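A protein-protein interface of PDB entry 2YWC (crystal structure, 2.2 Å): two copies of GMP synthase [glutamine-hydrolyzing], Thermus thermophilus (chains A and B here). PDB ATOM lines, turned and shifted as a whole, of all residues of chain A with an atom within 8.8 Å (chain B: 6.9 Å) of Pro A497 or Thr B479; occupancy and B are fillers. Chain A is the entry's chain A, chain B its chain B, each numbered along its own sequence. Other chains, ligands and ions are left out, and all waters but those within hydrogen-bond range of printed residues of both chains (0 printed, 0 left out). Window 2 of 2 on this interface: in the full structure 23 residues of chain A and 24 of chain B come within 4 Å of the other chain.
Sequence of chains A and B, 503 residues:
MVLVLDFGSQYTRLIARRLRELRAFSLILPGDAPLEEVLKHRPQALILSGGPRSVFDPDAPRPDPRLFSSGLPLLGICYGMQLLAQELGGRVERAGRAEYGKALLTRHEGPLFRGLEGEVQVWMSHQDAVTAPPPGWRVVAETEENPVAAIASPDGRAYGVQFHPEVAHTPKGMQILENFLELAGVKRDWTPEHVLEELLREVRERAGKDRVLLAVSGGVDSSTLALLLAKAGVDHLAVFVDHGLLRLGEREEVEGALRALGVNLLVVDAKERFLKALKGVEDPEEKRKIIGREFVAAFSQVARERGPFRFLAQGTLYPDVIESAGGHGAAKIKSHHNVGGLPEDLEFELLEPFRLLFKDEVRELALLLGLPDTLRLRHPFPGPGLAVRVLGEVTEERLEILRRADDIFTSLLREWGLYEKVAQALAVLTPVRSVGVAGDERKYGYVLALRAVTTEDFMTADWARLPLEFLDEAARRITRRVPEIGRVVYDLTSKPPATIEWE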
ATOM      1  N   ARG A 451      20.452 -13.067  13.866  1.00  0.00           N
ATOM      2  CA  ARG A 451      20.921 -11.832  13.271  1.00  0.00           C
ATOM      3  C   ARG A 451      21.531 -10.901  14.319  1.00  0.00           C
ATOM      4  O   ARG A 451      20.894 -10.578  15.328  1.00  0.00           O
ATOM      5  CB  ARG A 451      19.709 -11.190  12.583  1.00  0.00           C
ATOM      6  CG  ARG A 451      19.738  -9.705  12.272  1.00  0.00           C
ATOM      7  CD  ARG A 451      20.805  -9.537  11.187  1.00  0.00           C
ATOM      8  NE  ARG A 451      20.540  -8.386  10.348  1.00  0.00           N
ATOM      9  CZ  ARG A 451      21.351  -8.042   9.359  1.00  0.00           C
ATOM     10  NH1 ARG A 451      22.439  -8.775   9.145  1.00  0.00           N
ATOM     11  NH2 ARG A 451      21.076  -7.000   8.587  1.00  0.00           N
ATOM     12  N   MET A 459      22.706   3.085  10.901  1.00  0.00           N
ATOM     13  CA  MET A 459      22.323   3.718   9.642  1.00  0.00           C
ATOM     14  C   MET A 459      23.210   3.171   8.522  1.00  0.00           C
ATOM     15  O   MET A 459      22.775   3.024   7.379  1.00  0.00           O
ATOM     16  CB  MET A 459      22.457   5.238   9.767  1.00  0.00           C
ATOM     17  CG  MET A 459      21.129   5.939  10.056  1.00  0.00           C
ATOM     18  SD  MET A 459      21.308   7.673  10.563  1.00  0.00           S
ATOM     19  CE  MET A 459      22.267   8.345   9.177  1.00  0.00           C
ATOM     20  N   THR A 460      24.318   2.599   9.004  1.00  0.00           N
ATOM     21  CA  THR A 460      25.254   1.718   8.310  1.00  0.00           C
ATOM     22  C   THR A 460      25.600   0.683   9.368  1.00  0.00           C
ATOM     23  O   THR A 460      25.855   1.037  10.510  1.00  0.00           O
ATOM     24  CB  THR A 460      26.562   2.417   7.889  1.00  0.00           C
ATOM     25  OG1 THR A 460      27.115   3.111   9.014  1.00  0.00           O
ATOM     26  CG2 THR A 460      26.309   3.380   6.742  1.00  0.00           C
ATOM     27  N   ALA A 461      25.601  -0.588   9.002  1.00  0.00           N
ATOM     28  CA  ALA A 461      25.910  -1.622   9.972  1.00  0.00           C
ATOM     29  C   ALA A 461      26.511  -2.826   9.283  1.00  0.00           C
ATOM     30  O   ALA A 461      26.204  -3.099   8.128  1.00  0.00           O
ATOM     31  CB  ALA A 461      24.638  -2.031  10.722  1.00  0.00           C
ATOM     32  N   TRP A 463      27.321  -7.070   9.464  1.00  0.00           N
ATOM     33  CA  TRP A 463      26.846  -8.244  10.148  1.00  0.00           C
ATOM     34  C   TRP A 463      27.927  -8.604  11.172  1.00  0.00           C
ATOM     35  O   TRP A 463      29.120  -8.422  10.927  1.00  0.00           O
ATOM     36  CB  TRP A 463      26.550  -9.375   9.164  1.00  0.00           C
ATOM     37  CG  TRP A 463      27.693  -9.854   8.338  1.00  0.00           C
ATOM     38  CD1 TRP A 463      28.194  -9.275   7.211  1.00  0.00           C
ATOM     39  CD2 TRP A 463      28.447 -11.058   8.545  1.00  0.00           C
ATOM     40  NE1 TRP A 463      29.210 -10.050   6.698  1.00  0.00           N
ATOM     41  CE2 TRP A 463      29.383 -11.150   7.498  1.00  0.00           C
ATOM     42  CE3 TRP A 463      28.413 -12.071   9.517  1.00  0.00           C
ATOM     43  CZ2 TRP A 463      30.285 -12.213   7.391  1.00  0.00           C
ATOM     44  CZ3 TRP A 463      29.302 -13.126   9.417  1.00  0.00           C
ATOM     45  CH2 TRP A 463      30.229 -13.192   8.360  1.00  0.00           C
ATOM     46  N   ASP A 491      22.230 -14.551   9.379  1.00  0.00           N
ATOM     47  CA  ASP A 491      22.182 -13.507   8.360  1.00  0.00           C
ATOM     48  C   ASP A 491      23.579 -12.938   8.071  1.00  0.00           C
ATOM     49  O   ASP A 491      24.263 -12.453   8.983  1.00  0.00           O
ATOM     50  CB  ASP A 491      21.255 -12.382   8.830  1.00  0.00           C
ATOM     51  CG  ASP A 491      20.869 -11.439   7.708  1.00  0.00           C
ATOM     52  OD1 ASP A 491      21.645 -11.320   6.731  1.00  0.00           O
ATOM     53  OD2 ASP A 491      19.795 -10.812   7.812  1.00  0.00           O
ATOM     54  N   LEU A 492      23.995 -12.981   6.806  1.00  0.00           N
ATOM     55  CA  LEU A 492      25.317 -12.484   6.429  1.00  0.00           C
ATOM     56  C   LEU A 492      25.293 -11.109   5.741  1.00  0.00           C
ATOM     57  O   LEU A 492      26.312 -10.641   5.229  1.00  0.00           O
ATOM     58  CB  LEU A 492      25.990 -13.480   5.495  1.00  0.00           C
ATOM     59  CG  LEU A 492      26.202 -14.903   6.014  1.00  0.00           C
ATOM     60  CD1 LEU A 492      26.655 -15.790   4.868  1.00  0.00           C
ATOM     61  CD2 LEU A 492      27.227 -14.891   7.148  1.00  0.00           C
ATOM     62  N   THR A 493      24.144 -10.452   5.759  1.00  0.00           N
ATOM     63  CA  THR A 493      24.008  -9.179   5.069  1.00  0.00           C
ATOM     64  C   THR A 493      24.200  -7.927   5.901  1.00  0.00           C
ATOM     65  O   THR A 493      23.598  -7.763   6.944  1.00  0.00           O
ATOM     66  CB  THR A 493      22.634  -9.081   4.385  1.00  0.00           C
ATOM     67  OG1 THR A 493      22.285 -10.357   3.842  1.00  0.00           O
ATOM     68  CG2 THR A 493      22.678  -8.065   3.262  1.00  0.00           C
ATOM     69  N   SER A 494      25.041  -7.037   5.402  1.00  0.00           N
ATOM     70  CA  SER A 494      25.304  -5.773   6.072  1.00  0.00           C
ATOM     71  C   SER A 494      24.316  -4.703   5.611  1.00  0.00           C
ATOM     72  O   SER A 494      23.438  -4.958   4.776  1.00  0.00           O
ATOM     73  CB  SER A 494      26.725  -5.300   5.757  1.00  0.00           C
ATOM     74  OG  SER A 494      27.687  -6.043   6.486  1.00  0.00           O
ATOM     75  N   LYS A 495      24.486  -3.502   6.150  1.00  0.00           N
ATOM     76  CA  LYS A 495      23.649  -2.365   5.797  1.00  0.00           C
ATOM     77  C   LYS A 495      24.522  -1.159   5.447  1.00  0.00           C
ATOM     78  O   LYS A 495      25.204  -0.619   6.309  1.00  0.00           O
ATOM     79  CB  LYS A 495      22.736  -1.981   6.956  1.00  0.00           C
ATOM     80  CG  LYS A 495      21.905  -0.730   6.670  1.00  0.00           C
ATOM     81  CD  LYS A 495      21.053  -0.326   7.869  1.00  0.00           C
ATOM     82  CE  LYS A 495      19.956   0.660   7.460  1.00  0.00           C
ATOM     83  NZ  LYS A 495      19.058   0.989   8.591  1.00  0.00           N
ATOM     84  N   PRO A 496      24.524  -0.734   4.171  1.00  0.00           N
ATOM     85  CA  PRO A 496      23.764  -1.319   3.058  1.00  0.00           C
ATOM     86  C   PRO A 496      24.296  -2.706   2.718  1.00  0.00           C
ATOM     87  O   PRO A 496      25.371  -3.087   3.173  1.00  0.00           O
ATOM     88  CB  PRO A 496      23.989  -0.317   1.925  1.00  0.00           C
ATOM     89  CG  PRO A 496      25.358   0.219   2.219  1.00  0.00           C
ATOM     90  CD  PRO A 496      25.293   0.439   3.716  1.00  0.00           C
ATOM     91  N   PRO A 497      23.579  -3.462   1.876  1.00  0.00           N
ATOM     92  CA  PRO A 497      22.319  -3.162   1.193  1.00  0.00           C
ATOM     93  C   PRO A 497      21.048  -3.553   1.919  1.00  0.00           C
ATOM     94  O   PRO A 497      19.959  -3.411   1.356  1.00  0.00           O
ATOM     95  CB  PRO A 497      22.441  -3.969  -0.073  1.00  0.00           C
ATOM     96  CG  PRO A 497      22.999  -5.269   0.503  1.00  0.00           C
ATOM     97  CD  PRO A 497      24.104  -4.758   1.413  1.00  0.00           C
ATOM     98  N   ALA A 498      21.161  -4.074   3.134  1.00  0.00           N
ATOM     99  CA  ALA A 498      19.961  -4.503   3.835  1.00  0.00           C
ATOM    100  C   ALA A 498      19.731  -3.854   5.179  1.00  0.00           C
ATOM    101  O   ALA A 498      20.658  -3.403   5.839  1.00  0.00           O
ATOM    102  CB  ALA A 498      19.967  -6.031   3.990  1.00  0.00           C
ATOM    103  N   THR A 499      18.471  -3.830   5.581  1.00  0.00           N
ATOM    104  CA  THR A 499      18.080  -3.258   6.858  1.00  0.00           C
ATOM    105  C   THR A 499      18.491  -4.188   7.998  1.00  0.00           C
ATOM    106  O   THR A 499      18.821  -5.354   7.774  1.00  0.00           O
ATOM    107  CB  THR A 499      16.564  -3.074   6.906  1.00  0.00           C
ATOM    108  OG1 THR A 499      15.935  -4.267   6.415  1.00  0.00           O
ATOM    109  CG2 THR A 499      16.141  -1.880   6.054  1.00  0.00           C
ATOM    110  N   ILE A 500      18.468  -3.679   9.220  1.00  0.00           N
ATOM    111  CA  ILE A 500      18.824  -4.504  10.361  1.00  0.00           C
ATOM    112  C   ILE A 500      17.692  -5.506  10.607  1.00  0.00           C
ATOM    113  O   ILE A 500      17.942  -6.704  10.713  1.00  0.00           O
ATOM    114  CB  ILE A 500      19.096  -3.632  11.608  1.00  0.00           C
ATOM    115  CG1 ILE A 500      20.354  -2.795  11.359  1.00  0.00           C
ATOM    116  CG2 ILE A 500      19.274  -4.517  12.843  1.00  0.00           C
ATOM    117  CD1 ILE A 500      20.825  -1.841  12.496  1.00  0.00           C
ATOM    118  N   ILE B 408      27.698 -18.244  -8.719  1.00  0.00           N
ATOM    119  CA  ILE B 408      28.625 -17.382  -7.991  1.00  0.00           C
ATOM    120  C   ILE B 408      29.205 -18.082  -6.752  1.00  0.00           C
ATOM    121  O   ILE B 408      30.409 -17.992  -6.476  1.00  0.00           O
ATOM    122  CB  ILE B 408      27.919 -16.065  -7.565  1.00  0.00           C
ATOM    123  CG1 ILE B 408      27.491 -15.285  -8.815  1.00  0.00           C
ATOM    124  CG2 ILE B 408      28.847 -15.210  -6.714  1.00  0.00           C
ATOM    125  CD1 ILE B 408      26.474 -14.173  -8.565  1.00  0.00           C
ATOM    126  N   ALA B 474      31.071 -13.901  -0.305  1.00  0.00           N
ATOM    127  CA  ALA B 474      29.983 -14.561  -1.010  1.00  0.00           C
ATOM    128  C   ALA B 474      28.674 -13.769  -0.926  1.00  0.00           C
ATOM    129  O   ALA B 474      27.972 -13.604  -1.926  1.00  0.00           O
ATOM    130  CB  ALA B 474      29.786 -15.982  -0.457  1.00  0.00           C
ATOM    131  N   ALA B 475      28.348 -13.276   0.265  1.00  0.00           N
ATOM    132  CA  ALA B 475      27.116 -12.518   0.455  1.00  0.00           C
ATOM    133  C   ALA B 475      27.115 -11.203  -0.333  1.00  0.00           C
ATOM    134  O   ALA B 475      26.102 -10.819  -0.909  1.00  0.00           O
ATOM    135  CB  ALA B 475      26.893 -12.241   1.944  1.00  0.00           C
ATOM    136  N   ARG B 476      28.244 -10.510  -0.343  1.00  0.00           N
ATOM    137  CA  ARG B 476      28.334  -9.256  -1.073  1.00  0.00           C
ATOM    138  C   ARG B 476      28.293  -9.462  -2.588  1.00  0.00           C
ATOM    139  O   ARG B 476      27.556  -8.767  -3.284  1.00  0.00           O
ATOM    140  CB  ARG B 476      29.595  -8.499  -0.668  1.00  0.00           C
ATOM    141  CG  ARG B 476      29.479  -7.864   0.711  1.00  0.00           C
ATOM    142  CD  ARG B 476      30.744  -7.136   1.083  1.00  0.00           C
ATOM    143  NE  ARG B 476      31.864  -8.060   1.154  1.00  0.00           N
ATOM    144  CZ  ARG B 476      33.137  -7.687   1.244  1.00  0.00           C
ATOM    145  NH1 ARG B 476      33.447  -6.395   1.271  1.00  0.00           N
ATOM    146  NH2 ARG B 476      34.098  -8.606   1.307  1.00  0.00           N
ATOM    147  N   ARG B 477      29.052 -10.427  -3.095  1.00  0.00           N
ATOM    148  CA  ARG B 477      29.069 -10.693  -4.530  1.00  0.00           C
ATOM    149  C   ARG B 477      27.663 -11.035  -5.032  1.00  0.00           C
ATOM    150  O   ARG B 477      27.240 -10.573  -6.093  1.00  0.00           O
ATOM    151  CB  ARG B 477      30.016 -11.851  -4.847  1.00  0.00           C
ATOM    152  CG  ARG B 477      30.323 -12.003  -6.325  1.00  0.00           C
ATOM    153  CD  ARG B 477      31.272 -10.919  -6.769  1.00  0.00           C
ATOM    154  NE  ARG B 477      32.644 -11.167  -6.331  1.00  0.00           N
ATOM    155  CZ  ARG B 477      33.423 -12.117  -6.843  1.00  0.00           C
ATOM    156  NH1 ARG B 477      32.960 -12.903  -7.807  1.00  0.00           N
ATOM    157  NH2 ARG B 477      34.664 -12.282  -6.398  1.00  0.00           N
ATOM    158  N   ILE B 478      26.940 -11.838  -4.256  1.00  0.00           N
ATOM    159  CA  ILE B 478      25.588 -12.242  -4.609  1.00  0.00           C
ATOM    160  C   ILE B 478      24.605 -11.073  -4.650  1.00  0.00           C
ATOM    161  O   ILE B 478      23.957 -10.867  -5.673  1.00  0.00           O
ATOM    162  CB  ILE B 478      25.069 -13.344  -3.649  1.00  0.00           C
ATOM    163  CG1 ILE B 478      25.836 -14.646  -3.923  1.00  0.00           C
ATOM    164  CG2 ILE B 478      23.563 -13.589  -3.853  1.00  0.00           C
ATOM    165  CD1 ILE B 478      25.437 -15.827  -3.038  1.00  0.00           C
ATOM    166  N   THR B 479      24.489 -10.300  -3.570  1.00  0.00           N
ATOM    167  CA  THR B 479      23.550  -9.178  -3.596  1.00  0.00           C
ATOM    168  C   THR B 479      23.920  -8.111  -4.637  1.00  0.00           C
ATOM    169  O   THR B 479      23.041  -7.439  -5.182  1.00  0.00           O
ATOM    170  CB  THR B 479      23.382  -8.505  -2.203  1.00  0.00           C
ATOM    171  OG1 THR B 479      24.658  -8.108  -1.682  1.00  0.00           O
ATOM    172  CG2 THR B 479      22.701  -9.463  -1.234  1.00  0.00           C
ATOM    173  N   ARG B 480      25.211  -7.973  -4.927  1.00  0.00           N
ATOM    174  CA  ARG B 480      25.680  -6.992  -5.907  1.00  0.00           C
ATOM    175  C   ARG B 480      25.379  -7.408  -7.349  1.00  0.00           C
ATOM    176  O   ARG B 480      24.854  -6.617  -8.129  1.00  0.00           O
ATOM    177  CB  ARG B 480      27.190  -6.758  -5.751  1.00  0.00           C
ATOM    178  CG  ARG B 480      27.789  -5.819  -6.791  1.00  0.00           C
ATOM    179  CD  ARG B 480      29.252  -5.473  -6.490  1.00  0.00           C
ATOM    180  NE  ARG B 480      30.136  -6.643  -6.491  1.00  0.00           N
ATOM    181  CZ  ARG B 480      30.672  -7.194  -5.402  1.00  0.00           C
ATOM    182  NH1 ARG B 480      30.422  -6.691  -4.198  1.00  0.00           N
ATOM    183  NH2 ARG B 480      31.467  -8.251  -5.515  1.00  0.00           N
ATOM    184  N   ARG B 481      25.705  -8.656  -7.682  1.00  0.00           N
ATOM    185  CA  ARG B 481      25.506  -9.203  -9.020  1.00  0.00           C
ATOM    186  C   ARG B 481      24.101  -9.767  -9.248  1.00  0.00           C
ATOM    187  O   ARG B 481      23.685  -9.945 -10.386  1.00  0.00           O
ATOM    188  CB  ARG B 481      26.544 -10.298  -9.281  1.00  0.00           C
ATOM    189  CG  ARG B 481      27.977  -9.924  -8.892  1.00  0.00           C
ATOM    190  CD  ARG B 481      28.737  -9.247 -10.019  1.00  0.00           C
ATOM    191  NE  ARG B 481      29.961  -9.983 -10.338  1.00  0.00           N
ATOM    192  CZ  ARG B 481      31.130  -9.820  -9.719  1.00  0.00           C
ATOM    193  NH1 ARG B 481      31.252  -8.930  -8.742  1.00  0.00           N
ATOM    194  NH2 ARG B 481      32.174 -10.566 -10.067  1.00  0.00           N
ATOM    195  N   VAL B 482      23.368 -10.062  -8.180  1.00  0.00           N
ATOM    196  CA  VAL B 482      22.017 -10.588  -8.333  1.00  0.00           C
ATOM    197  C   VAL B 482      21.038  -9.748  -7.508  1.00  0.00           C
ATOM    198  O   VAL B 482      20.489 -10.206  -6.503  1.00  0.00           O
ATOM    199  CB  VAL B 482      21.933 -12.064  -7.902  1.00  0.00           C
ATOM    200  CG1 VAL B 482      20.557 -12.618  -8.210  1.00  0.00           C
ATOM    201  CG2 VAL B 482      22.980 -12.873  -8.629  1.00  0.00           C
ATOM    202  N   PRO B 483      20.797  -8.502  -7.950  1.00  0.00           N
ATOM    203  CA  PRO B 483      19.920  -7.482  -7.363  1.00  0.00           C
ATOM    204  C   PRO B 483      18.566  -7.917  -6.796  1.00  0.00           C
ATOM    205  O   PRO B 483      18.037  -7.263  -5.905  1.00  0.00           O
ATOM    206  CB  PRO B 483      19.771  -6.472  -8.498  1.00  0.00           C
ATOM    207  CG  PRO B 483      21.099  -6.540  -9.165  1.00  0.00           C
ATOM    208  CD  PRO B 483      21.313  -8.031  -9.251  1.00  0.00           C
ATOM    209  N   GLU B 484      17.991  -8.992  -7.316  1.00  0.00           N
ATOM    210  CA  GLU B 484      16.708  -9.454  -6.792  1.00  0.00           C
ATOM    211  C   GLU B 484      16.881 -10.180  -5.461  1.00  0.00           C
ATOM    212  O   GLU B 484      15.902 -10.473  -4.774  1.00  0.00           O
ATOM    213  CB  GLU B 484      16.013 -10.375  -7.793  1.00  0.00           C
ATOM    214  CG  GLU B 484      16.971 -11.171  -8.631  1.00  0.00           C
ATOM    215  CD  GLU B 484      17.476 -10.385  -9.811  1.00  0.00           C
ATOM    216  OE1 GLU B 484      16.683 -10.168 -10.750  1.00  0.00           O
ATOM    217  OE2 GLU B 484      18.655  -9.977  -9.800  1.00  0.00           O
ATOM    218  N   ILE B 485      18.128 -10.492  -5.116  1.00  0.00           N
ATOM    219  CA  ILE B 485      18.436 -11.157  -3.850  1.00  0.00           C
ATOM    220  C   ILE B 485      18.778 -10.021  -2.892  1.00  0.00           C
ATOM    221  O   ILE B 485      19.821  -9.378  -3.029  1.00  0.00           O
ATOM    222  CB  ILE B 485      19.677 -12.084  -3.946  1.00  0.00           C
ATOM    223  CG1 ILE B 485      19.489 -13.154  -5.032  1.00  0.00           C
ATOM    224  CG2 ILE B 485      19.944 -12.718  -2.586  1.00  0.00           C
ATOM    225  CD1 ILE B 485      19.004 -14.553  -4.571  1.00  0.00           C
ATOM    226  N   GLY B 486      17.900  -9.765  -1.934  1.00  0.00           N
ATOM    227  CA  GLY B 486      18.149  -8.689  -0.991  1.00  0.00           C
ATOM    228  C   GLY B 486      18.857  -9.107   0.289  1.00  0.00           C
ATOM    229  O   GLY B 486      19.381  -8.261   1.022  1.00  0.00           O
ATOM    230  N   ARG B 487      18.883 -10.411   0.558  1.00  0.00           N
ATOM    231  CA  ARG B 487      19.502 -10.916   1.769  1.00  0.00           C
ATOM    232  C   ARG B 487      20.092 -12.317   1.579  1.00  0.00           C
ATOM    233  O   ARG B 487      19.462 -13.199   0.978  1.00  0.00           O
ATOM    234  CB  ARG B 487      18.457 -10.925   2.887  1.00  0.00           C
ATOM    235  CG  ARG B 487      19.034 -10.988   4.287  1.00  0.00           C
ATOM    236  CD  ARG B 487      17.946 -10.872   5.338  1.00  0.00           C
ATOM    237  NE  ARG B 487      17.306  -9.553   5.382  1.00  0.00           N
ATOM    238  CZ  ARG B 487      17.759  -8.494   6.055  1.00  0.00           C
ATOM    239  NH1 ARG B 487      18.884  -8.562   6.765  1.00  0.00           N
ATOM    240  NH2 ARG B 487      17.059  -7.360   6.041  1.00  0.00           N
ATOM    241  N   VAL B 488      21.311 -12.504   2.077  1.00  0.00           N
ATOM    242  CA  VAL B 488      21.991 -13.787   2.003  1.00  0.00           C
ATOM    243  C   VAL B 488      22.168 -14.340   3.410  1.00  0.00           C
ATOM    244  O   VAL B 488      22.607 -13.643   4.328  1.00  0.00           O
ATOM    245  CB  VAL B 488      23.353 -13.664   1.314  1.00  0.00           C
ATOM    246  CG1 VAL B 488      24.040 -15.037   1.259  1.00  0.00           C
ATOM    247  CG2 VAL B 488      23.154 -13.109  -0.096  1.00  0.00           C
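No position is printed for both chains.
Of the 12 pairs that touch across the chains among the printed residues, none has its exchanged pair printed and touching as well.
The guanidinium group (NH1) of Arg A451 is in hydrogen-bond range of the backbone carbonyl oxygen (O) of Thr A493 (2.7 Å).
The backbone carbonyl oxygen (O) of Thr A499 sits at hydrogen-bond distance from the guanidinium group (NH2) of Arg A451 (2.9 Å).
The indole nitrogen (NE1) of Trp A463 lies close to the backbone carbonyl oxygen (O) of Leu A492 (3.3 Å).
OD1 of Asp A491 is in hydrogen-bond range of N of Thr A493, at 2.8 Å.
The backbone carbonyl oxygen (O) of Ala B475 is in hydrogen-bond range of the side-chain hydroxyl (OG1) of Thr B479 (3.2 Å).
O of Arg B476 lies within hydrogen-bond range of OG1 of Thr B479, 3.4 Å away.
The guanidinium group of Arg B487 lies within salt-bridge range of the side-chain carboxylate of Asp A491, 2.6 Å away.
N of Leu A492 lies within hydrogen-bond range of O of Val B488 (2.9 Å).
The side-chain hydroxyl (OG1) of Thr A493 sits at hydrogen-bond distance from the backbone NH (N) of Val B488, at 2.9 Å.
NH2 of Arg B487 lies within hydrogen-bond range of O of Thr A499, at 3.2 Å.
The guanidinium group (NH1) of Arg B487 lies close to the guanidinium group (NH2) of Arg A451 (3.3 Å).
O of Val B488 sits close to OD1 of Asp A491, at 3.5 Å.
Pro A497 touches one residue of chain B.
Printed residues of chain B within 4 Å of Ala A498: Gly B486 and Arg B487.
Printed residues of chain B within 4 Å of Asp A491: Arg B487 and Val B488.
Of the printed residues of chain A, Gly B486 touches Thr A493 and Ala A498.
Of the printed residues of chain A, Val B488 touches Asp A491 (3.5 Å), Leu A492 (2.9 Å) and Thr A493 (2.9 Å).
Of the printed residues of chain B, Arg A451 touches Arg B487 (3.3 Å).
The nearest residue of chain B that does not touch Pro A497 is Gly B486 (4.7 Å).
The nearest printed residue of chain A that does not touch Arg B487 is Ile A500 (4.5 Å).
Of the 16 printed residues of chain B, 5 touch a printed residue of chain A.
Along chain B the printed residues that touch a printed residue of chain A span positions 475 to 488.
Among the printed residues, 12 pairs touch across the chains.
O of Leu A492 touches CB of Ala B475 (3.7 Å).
O of Gly B486 touches CG2 of Thr A493, at 3.99 Å.
Thr A493 touches Arg B487.
CG of Pro A497 touches OG1 of Thr B479 (3.9 Å).
Gly B486 touches Ala A498.
Arg B487 touches Ala A498 (NH2 to CB, 3.8 Å).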
